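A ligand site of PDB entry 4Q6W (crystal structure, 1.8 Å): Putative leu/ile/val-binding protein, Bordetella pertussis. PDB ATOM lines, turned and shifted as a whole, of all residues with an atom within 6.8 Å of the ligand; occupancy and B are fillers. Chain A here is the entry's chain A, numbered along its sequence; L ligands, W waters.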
ATOM      1  N   PHE A  45      -3.846  -5.799 -14.257  1.00  0.00           N
ATOM      2  CA  PHE A  45      -4.901  -4.835 -13.930  1.00  0.00           C
ATOM      3  C   PHE A  45      -4.880  -3.554 -14.764  1.00  0.00           C
ATOM      4  O   PHE A  45      -5.917  -3.111 -15.259  1.00  0.00           O
ATOM      5  CB  PHE A  45      -4.843  -4.491 -12.429  1.00  0.00           C
ATOM      6  CG  PHE A  45      -5.056  -5.696 -11.557  1.00  0.00           C
ATOM      7  CD1 PHE A  45      -6.303  -6.286 -11.463  1.00  0.00           C
ATOM      8  CD2 PHE A  45      -4.007  -6.266 -10.883  1.00  0.00           C
ATOM      9  CE1 PHE A  45      -6.495  -7.409 -10.698  1.00  0.00           C
ATOM     10  CE2 PHE A  45      -4.189  -7.404 -10.130  1.00  0.00           C
ATOM     11  CZ  PHE A  45      -5.441  -7.972 -10.029  1.00  0.00           C
ATOM     12  N   LEU A  81       1.583   0.034 -10.191  1.00  0.00           N
ATOM     13  CA  LEU A  81       1.008  -0.295  -8.873  1.00  0.00           C
ATOM     14  C   LEU A  81       1.860   0.263  -7.720  1.00  0.00           C
ATOM     15  O   LEU A  81       1.722  -0.175  -6.566  1.00  0.00           O
ATOM     16  CB  LEU A  81       0.775  -1.809  -8.707  1.00  0.00           C
ATOM     17  CG  LEU A  81      -0.389  -2.186  -7.795  1.00  0.00           C
ATOM     18  CD1 LEU A  81      -1.671  -2.238  -8.612  1.00  0.00           C
ATOM     19  CD2 LEU A  81      -0.149  -3.513  -7.051  1.00  0.00           C
ATOM     20  N   ALA A 106      -5.120   0.995 -10.337  1.00  0.00           N
ATOM     21  CA  ALA A 106      -5.350  -0.203  -9.558  1.00  0.00           C
ATOM     22  C   ALA A 106      -4.564  -0.061  -8.286  1.00  0.00           C
ATOM     23  O   ALA A 106      -3.546   0.614  -8.241  1.00  0.00           O
ATOM     24  CB  ALA A 106      -4.885  -1.449 -10.334  1.00  0.00           C
ATOM     25  N   GLY A 107      -4.993  -0.766  -7.239  1.00  0.00           N
ATOM     26  CA  GLY A 107      -4.139  -0.899  -6.083  1.00  0.00           C
ATOM     27  C   GLY A 107      -4.484   0.083  -4.970  1.00  0.00           C
ATOM     28  O   GLY A 107      -4.528   1.322  -5.174  1.00  0.00           O
ATOM     29  N   SER A 108      -4.767  -0.470  -3.808  1.00  0.00           N
ATOM     30  CA  SER A 108      -5.090   0.327  -2.658  1.00  0.00           C
ATOM     31  C   SER A 108      -3.919   1.235  -2.259  1.00  0.00           C
ATOM     32  O   SER A 108      -4.137   2.352  -1.798  1.00  0.00           O
ATOM     33  CB  SER A 108      -5.507  -0.588  -1.495  1.00  0.00           C
ATOM     34  OG  SER A 108      -6.813  -1.113  -1.727  1.00  0.00           O
ATOM     35  N   GLY A 109      -2.683   0.749  -2.381  1.00  0.00           N
ATOM     36  CA  GLY A 109      -1.520   1.577  -2.073  1.00  0.00           C
ATOM     37  C   GLY A 109      -1.502   2.875  -2.883  1.00  0.00           C
ATOM     38  O   GLY A 109      -1.520   3.966  -2.311  1.00  0.00           O
ATOM     39  N   PRO A 110      -1.428   2.758  -4.213  1.00  0.00           N
ATOM     40  CA  PRO A 110      -1.517   3.950  -5.068  1.00  0.00           C
ATOM     41  C   PRO A 110      -2.766   4.792  -4.795  1.00  0.00           C
ATOM     42  O   PRO A 110      -2.611   5.996  -4.671  1.00  0.00           O
ATOM     43  CB  PRO A 110      -1.569   3.352  -6.485  1.00  0.00           C
ATOM     44  CG  PRO A 110      -0.700   2.105  -6.342  1.00  0.00           C
ATOM     45  CD  PRO A 110      -1.058   1.547  -4.974  1.00  0.00           C
ATOM     46  N   ILE A 129     -10.780  -0.531  -9.258  1.00  0.00           N
ATOM     47  CA  ILE A 129     -10.300  -1.804  -8.702  1.00  0.00           C
ATOM     48  C   ILE A 129     -10.062  -1.837  -7.184  1.00  0.00           C
ATOM     49  O   ILE A 129     -10.490  -2.795  -6.523  1.00  0.00           O
ATOM     50  CB  ILE A 129      -9.000  -2.255  -9.401  1.00  0.00           C
ATOM     51  CG1 ILE A 129      -9.260  -2.466 -10.894  1.00  0.00           C
ATOM     52  CG2 ILE A 129      -8.501  -3.516  -8.765  1.00  0.00           C
ATOM     53  CD1 ILE A 129      -8.039  -2.843 -11.690  1.00  0.00           C
ATOM     54  N   ALA A 130      -9.389  -0.824  -6.649  1.00  0.00           N
ATOM     55  CA  ALA A 130      -8.950  -0.830  -5.254  1.00  0.00           C
ATOM     56  C   ALA A 130     -10.079  -1.174  -4.276  1.00  0.00           C
ATOM     57  O   ALA A 130     -11.140  -0.542  -4.316  1.00  0.00           O
ATOM     58  CB  ALA A 130      -8.318   0.511  -4.898  1.00  0.00           C
ATOM     59  N   GLN A 131      -9.846  -2.144  -3.394  1.00  0.00           N
ATOM     60  CA  GLN A 131     -10.925  -2.714  -2.581  1.00  0.00           C
ATOM     61  C   GLN A 131     -10.990  -2.224  -1.136  1.00  0.00           C
ATOM     62  O   GLN A 131     -11.906  -2.592  -0.391  1.00  0.00           O
ATOM     63  CB  GLN A 131     -10.835  -4.259  -2.585  1.00  0.00           C
ATOM     64  CG  GLN A 131     -10.869  -4.864  -3.994  1.00  0.00           C
ATOM     65  CD  GLN A 131     -11.259  -6.367  -4.001  1.00  0.00           C
ATOM     66  OE1 GLN A 131     -11.569  -6.969  -2.966  1.00  0.00           O
ATOM     67  NE2 GLN A 131     -11.282  -6.937  -5.175  1.00  0.00           N
ATOM     68  N   THR A 132     -10.032  -1.418  -0.720  1.00  0.00           N
ATOM     69  CA  THR A 132     -10.069  -0.868   0.635  1.00  0.00           C
ATOM     70  C   THR A 132     -11.222   0.147   0.744  1.00  0.00           C
ATOM     71  O   THR A 132     -11.237   1.121   0.016  1.00  0.00           O
ATOM     72  CB  THR A 132      -8.754  -0.191   0.980  1.00  0.00           C
ATOM     73  OG1 THR A 132      -7.738  -1.192   1.022  1.00  0.00           O
ATOM     74  CG2 THR A 132      -8.849   0.470   2.337  1.00  0.00           C
ATOM     75  N   LEU A 155     -14.955  -4.429  -6.090  1.00  0.00           N
ATOM     76  CA  LEU A 155     -15.595  -5.249  -5.105  1.00  0.00           C
ATOM     77  C   LEU A 155     -14.946  -4.867  -3.784  1.00  0.00           C
ATOM     78  O   LEU A 155     -13.798  -5.230  -3.534  1.00  0.00           O
ATOM     79  CB  LEU A 155     -15.350  -6.733  -5.422  1.00  0.00           C
ATOM     80  CG  LEU A 155     -15.657  -7.757  -4.330  1.00  0.00           C
ATOM     81  CD1 LEU A 155     -17.142  -7.756  -3.969  1.00  0.00           C
ATOM     82  CD2 LEU A 155     -15.194  -9.174  -4.798  1.00  0.00           C
ATOM     83  N   ASN A 157     -13.681  -4.794   0.058  1.00  0.00           N
ATOM     84  CA  ASN A 157     -13.308  -5.829   1.013  1.00  0.00           C
ATOM     85  C   ASN A 157     -14.381  -6.241   2.009  1.00  0.00           C
ATOM     86  O   ASN A 157     -14.479  -7.403   2.329  1.00  0.00           O
ATOM     87  CB  ASN A 157     -12.068  -5.394   1.797  1.00  0.00           C
ATOM     88  CG  ASN A 157     -10.802  -5.723   1.057  1.00  0.00           C
ATOM     89  OD1 ASN A 157     -10.837  -6.468   0.070  1.00  0.00           O
ATOM     90  ND2 ASN A 157      -9.670  -5.200   1.545  1.00  0.00           N
ATOM     91  N   GLU A 160     -16.685  -8.508  -0.242  1.00  0.00           N
ATOM     92  CA  GLU A 160     -16.114  -9.812  -0.570  1.00  0.00           C
ATOM     93  C   GLU A 160     -16.012 -10.723   0.665  1.00  0.00           C
ATOM     94  O   GLU A 160     -16.169 -11.940   0.562  1.00  0.00           O
ATOM     95  CB  GLU A 160     -14.732  -9.668  -1.182  1.00  0.00           C
ATOM     96  CG  GLU A 160     -14.107 -11.013  -1.599  1.00  0.00           C
ATOM     97  CD  GLU A 160     -12.813 -10.876  -2.400  1.00  0.00           C
ATOM     98  OE1 GLU A 160     -12.295  -9.747  -2.532  1.00  0.00           O
ATOM     99  OE2 GLU A 160     -12.316 -11.897  -2.902  1.00  0.00           O
ATOM    100  N   GLU A 180      -0.894  -9.840   1.897  1.00  0.00           N
ATOM    101  CA  GLU A 180       0.115  -8.866   1.480  1.00  0.00           C
ATOM    102  C   GLU A 180       0.056  -7.663   2.413  1.00  0.00           C
ATOM    103  O   GLU A 180      -1.019  -7.299   2.923  1.00  0.00           O
ATOM    104  CB  GLU A 180      -0.122  -8.409   0.040  1.00  0.00           C
ATOM    105  CG  GLU A 180      -1.380  -7.549  -0.159  1.00  0.00           C
ATOM    106  CD  GLU A 180      -1.427  -6.911  -1.562  1.00  0.00           C
ATOM    107  OE1 GLU A 180      -2.075  -5.846  -1.726  1.00  0.00           O
ATOM    108  OE2 GLU A 180      -0.779  -7.467  -2.484  1.00  0.00           O
ATOM    109  N   THR A 182      -0.383  -4.514   2.487  1.00  0.00           N
ATOM    110  CA  THR A 182      -0.925  -3.257   2.011  1.00  0.00           C
ATOM    111  C   THR A 182      -2.250  -3.111   2.704  1.00  0.00           C
ATOM    112  O   THR A 182      -2.682  -4.034   3.413  1.00  0.00           O
ATOM    113  CB  THR A 182      -1.184  -3.265   0.471  1.00  0.00           C
ATOM    114  OG1 THR A 182      -2.200  -4.228   0.175  1.00  0.00           O
ATOM    115  CG2 THR A 182       0.077  -3.590  -0.310  1.00  0.00           C
ATOM    116  N   ALA A 183      -2.928  -1.976   2.488  1.00  0.00           N
ATOM    117  CA  ALA A 183      -4.255  -1.801   3.073  1.00  0.00           C
ATOM    118  C   ALA A 183      -5.233  -2.828   2.531  1.00  0.00           C
ATOM    119  O   ALA A 183      -6.138  -3.253   3.243  1.00  0.00           O
ATOM    120  CB  ALA A 183      -4.758  -0.389   2.835  1.00  0.00           C
ATOM    121  N   TYR A 184      -5.066  -3.225   1.275  1.00  0.00           N
ATOM    122  CA  TYR A 184      -5.893  -4.302   0.709  1.00  0.00           C
ATOM    123  C   TYR A 184      -5.745  -5.551   1.562  1.00  0.00           C
ATOM    124  O   TYR A 184      -6.748  -6.152   1.984  1.00  0.00           O
ATOM    125  CB  TYR A 184      -5.432  -4.594  -0.729  1.00  0.00           C
ATOM    126  CG  TYR A 184      -6.083  -5.800  -1.407  1.00  0.00           C
ATOM    127  CD1 TYR A 184      -7.463  -6.025  -1.343  1.00  0.00           C
ATOM    128  CD2 TYR A 184      -5.313  -6.663  -2.182  1.00  0.00           C
ATOM    129  CE1 TYR A 184      -8.049  -7.136  -2.021  1.00  0.00           C
ATOM    130  CE2 TYR A 184      -5.881  -7.734  -2.863  1.00  0.00           C
ATOM    131  CZ  TYR A 184      -7.237  -7.988  -2.775  1.00  0.00           C
ATOM    132  OH  TYR A 184      -7.731  -9.070  -3.477  1.00  0.00           O
ATOM    133  N   GLY A 185      -4.508  -5.938   1.825  1.00  0.00           N
ATOM    134  CA  GLY A 185      -4.237  -7.102   2.665  1.00  0.00           C
ATOM    135  C   GLY A 185      -4.663  -6.890   4.103  1.00  0.00           C
ATOM    136  O   GLY A 185      -5.301  -7.753   4.725  1.00  0.00           O
ATOM    137  N   GLN A 212       4.623  -7.495  -1.071  1.00  0.00           N
ATOM    138  CA  GLN A 212       4.444  -7.774  -2.495  1.00  0.00           C
ATOM    139  C   GLN A 212       5.802  -8.084  -3.128  1.00  0.00           C
ATOM    140  O   GLN A 212       6.782  -7.370  -2.892  1.00  0.00           O
ATOM    141  CB  GLN A 212       3.788  -6.584  -3.218  1.00  0.00           C
ATOM    142  CG  GLN A 212       2.293  -6.413  -2.881  1.00  0.00           C
ATOM    143  CD  GLN A 212       1.601  -5.305  -3.661  1.00  0.00           C
ATOM    144  OE1 GLN A 212       2.219  -4.289  -4.072  1.00  0.00           O
ATOM    145  NE2 GLN A 212       0.287  -5.485  -3.881  1.00  0.00           N
ATOM    146  N   GLY A 236      -4.332 -11.079  -1.477  1.00  0.00           N
ATOM    147  CA  GLY A 236      -3.202 -10.542  -2.223  1.00  0.00           C
ATOM    148  C   GLY A 236      -3.397 -10.802  -3.699  1.00  0.00           C
ATOM    149  O   GLY A 236      -4.519 -11.066  -4.138  1.00  0.00           O
ATOM    150  N   LEU A 237      -2.318 -10.732  -4.473  1.00  0.00           N
ATOM    151  CA  LEU A 237      -2.439 -10.817  -5.919  1.00  0.00           C
ATOM    152  C   LEU A 237      -1.773 -12.069  -6.510  1.00  0.00           C
ATOM    153  O   LEU A 237      -1.037 -12.779  -5.815  1.00  0.00           O
ATOM    154  CB  LEU A 237      -1.919  -9.537  -6.580  1.00  0.00           C
ATOM    155  CG  LEU A 237      -2.521  -8.268  -5.958  1.00  0.00           C
ATOM    156  CD1 LEU A 237      -1.894  -7.008  -6.558  1.00  0.00           C
ATOM    157  CD2 LEU A 237      -4.038  -8.250  -6.070  1.00  0.00           C
ATOM    158  N   SER A 260      -8.373 -14.296  -2.445  1.00  0.00           N
ATOM    159  CA  SER A 260      -9.222 -13.159  -2.840  1.00  0.00           C
ATOM    160  C   SER A 260      -9.358 -13.130  -4.383  1.00  0.00           C
ATOM    161  O   SER A 260      -8.504 -13.642  -5.080  1.00  0.00           O
ATOM    162  CB  SER A 260      -8.597 -11.855  -2.335  1.00  0.00           C
ATOM    163  OG  SER A 260      -7.225 -11.783  -2.685  1.00  0.00           O
ATOM    164  N   ASN A 261     -10.441 -12.507  -4.863  1.00  0.00           N
ATOM    165  CA  ASN A 261     -10.751 -12.361  -6.284  1.00  0.00           C
ATOM    166  C   ASN A 261      -9.572 -11.830  -7.071  1.00  0.00           C
ATOM    167  O   ASN A 261      -9.258 -12.336  -8.147  1.00  0.00           O
ATOM    168  CB  ASN A 261     -11.932 -11.385  -6.435  1.00  0.00           C
ATOM    169  CG  ASN A 261     -12.645 -11.474  -7.800  1.00  0.00           C
ATOM    170  OD1 ASN A 261     -13.758 -10.945  -7.906  1.00  0.00           O
ATOM    171  ND2 ASN A 261     -12.045 -12.132  -8.825  1.00  0.00           N
ATOM    172  N   GLY A 262      -8.917 -10.803  -6.535  1.00  0.00           N
ATOM    173  CA  GLY A 262      -7.803 -10.199  -7.258  1.00  0.00           C
ATOM    174  C   GLY A 262      -6.572 -11.087  -7.450  1.00  0.00           C
ATOM    175  O   GLY A 262      -5.652 -10.724  -8.178  1.00  0.00           O
ATOM    176  N   ALA A 263      -6.551 -12.251  -6.795  1.00  0.00           N
ATOM    177  CA  ALA A 263      -5.371 -13.110  -6.890  1.00  0.00           C
ATOM    178  C   ALA A 263      -5.527 -14.214  -7.902  1.00  0.00           C
ATOM    179  O   ALA A 263      -4.564 -14.904  -8.226  1.00  0.00           O
ATOM    180  CB  ALA A 263      -5.037 -13.692  -5.560  1.00  0.00           C
ATOM    181  N   PHE A 322     -11.959 -14.100 -14.335  1.00  0.00           N
ATOM    182  CA  PHE A 322     -11.081 -13.034 -13.904  1.00  0.00           C
ATOM    183  C   PHE A 322     -11.128 -11.789 -14.781  1.00  0.00           C
ATOM    184  O   PHE A 322     -10.662 -10.729 -14.374  1.00  0.00           O
ATOM    185  CB  PHE A 322      -9.649 -13.593 -13.758  1.00  0.00           C
ATOM    186  CG  PHE A 322      -8.682 -12.646 -13.073  1.00  0.00           C
ATOM    187  CD1 PHE A 322      -8.636 -12.551 -11.690  1.00  0.00           C
ATOM    188  CD2 PHE A 322      -7.828 -11.841 -13.829  1.00  0.00           C
ATOM    189  CE1 PHE A 322      -7.749 -11.684 -11.066  1.00  0.00           C
ATOM    190  CE2 PHE A 322      -6.936 -10.961 -13.202  1.00  0.00           C
ATOM    191  CZ  PHE A 322      -6.907 -10.888 -11.829  1.00  0.00           C
ATOM    192  N   ILE A 325     -12.493  -8.615 -13.010  1.00  0.00           N
ATOM    193  CA  ILE A 325     -11.772  -7.788 -12.051  1.00  0.00           C
ATOM    194  C   ILE A 325     -10.531  -7.163 -12.690  1.00  0.00           C
ATOM    195  O   ILE A 325      -9.931  -6.240 -12.159  1.00  0.00           O
ATOM    196  CB  ILE A 325     -11.486  -8.563 -10.749  1.00  0.00           C
ATOM    197  CG1 ILE A 325     -11.195  -7.589  -9.580  1.00  0.00           C
ATOM    198  CG2 ILE A 325     -10.391  -9.581 -10.947  1.00  0.00           C
ATOM    199  CD1 ILE A 325     -11.291  -8.276  -8.192  1.00  0.00           C
ATOM    200  N   ASN A 329     -14.397  -4.115 -15.040  1.00  0.00           N
ATOM    201  CA  ASN A 329     -14.557  -3.045 -14.059  1.00  0.00           C
ATOM    202  C   ASN A 329     -14.157  -1.682 -14.680  1.00  0.00           C
ATOM    203  O   ASN A 329     -14.853  -0.680 -14.481  1.00  0.00           O
ATOM    204  CB  ASN A 329     -13.871  -3.333 -12.684  1.00  0.00           C
ATOM    205  CG  ASN A 329     -12.454  -3.868 -12.815  1.00  0.00           C
ATOM    206  OD1 ASN A 329     -11.875  -3.871 -13.895  1.00  0.00           O
ATOM    207  ND2 ASN A 329     -11.920  -4.401 -11.724  1.00  0.00           N
HETATM  208  C1  LIG L   1      -6.164  -3.559  -4.080  1.00  0.00           C
HETATM  209  O1  LIG L   1      -5.004  -3.161  -3.821  1.00  0.00           O
HETATM  210  O2  LIG L   1      -7.149  -3.199  -3.397  1.00  0.00           O
HETATM  211  C2  LIG L   1      -6.409  -4.485  -5.255  1.00  0.00           C
HETATM  212  C3  LIG L   1      -7.535  -5.283  -5.222  1.00  0.00           C
HETATM  213  C4  LIG L   1      -7.800  -6.159  -6.298  1.00  0.00           C
HETATM  214  C5  LIG L   1      -6.941  -6.226  -7.390  1.00  0.00           C
HETATM  215  C6  LIG L   1      -5.794  -5.423  -7.412  1.00  0.00           C
HETATM  216  C7  LIG L   1      -5.533  -4.560  -6.339  1.00  0.00           C
HETATM  217  O3  LIG L   1      -8.926  -6.951  -6.258  1.00  0.00           O
HETATM  218  O   HOH W   1      -2.537  -4.200  -3.896  1.00  0.00           O
HETATM  219  O   HOH W   2     -10.246  -9.383  -4.486  1.00  0.00           O
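The side-chain carboxylate of Glu 160 lies close to the side-chain amide oxygen of Gln 131 (2.9 Å).
The side-chain hydroxyl (OG1) of Thr 182 sits close to the backbone NH (N) of Tyr 184 (3.2 Å).
The side-chain hydroxyl (OG1) of Thr 132 lies within hydrogen-bond range of the backbone NH (N) of Tyr 184 (3.4 Å).
OH of Tyr 184 is in hydrogen-bond range of OG of Ser 260.
The side-chain amide nitrogen (ND2) of Asn 157 lies within hydrogen-bond range of the backbone carbonyl oxygen (O) of Tyr 184.
O of Leu 155 sits close to OE1 of Gln 131 (2.9 Å).
The side-chain hydroxyl of Ser 108 lies within hydrogen-bond range of the side-chain hydroxyl of Thr 132.
The side-chain amide nitrogen (ND2) of Asn 329 lies within hydrogen-bond range of the backbone carbonyl oxygen (O) of Ile 325.
An oxygen (O3) of the ligand sits at hydrogen-bond distance from the side-chain amide nitrogen (NE2) of Gln 131, 2.6 Å away.
An oxygen (O1) of the ligand is in hydrogen-bond range of the backbone NH of Ser 108 (2.7 Å).
An oxygen (O2) of the ligand is in hydrogen-bond range of the backbone NH of Gln 131, at 2.9 Å.
The side-chain hydroxyl (OG) of Ser 108 sits at hydrogen-bond distance from an oxygen (O2) of the ligand (2.7 Å).
CZ of Phe 45 touches C5 of the ligand, 3.5 Å away.
Gly 107 touches the ligand.
CG2 of Ile 129 touches C5 of the ligand (3.4 Å).
CA of Ala 130 touches O2 of the ligand (3.5 Å).
Tyr 184 touches the ligand (CB to O1, 3.4 Å).
CD2 of Leu 237 touches C6 of the ligand, 3.6 Å away.
Gly 262 touches the ligand (CA to O3, 3.6 Å).
Ile 325 touches the ligand.
Hydrophobic or aromatic side chains within 4 Å of the ligand: Phe 45, Ile 129, Tyr 184, Leu 237 and Ile 325.
Within 4 Å of the ligand: Phe 45, Gly 107, Ser 108, Ile 129, Ala 130, Gln 131, Tyr 184, Leu 237, Gly 262 and Ile 325.
The nearest printed residue that does not touch the ligand is Thr 132 (4.3 Å).
Water W1 lies within hydrogen-bond range of O1 of the ligand (2.7 Å), OE1 of Glu 180 (2.8 Å) and NE2 of Gln 212 (3.1 Å).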
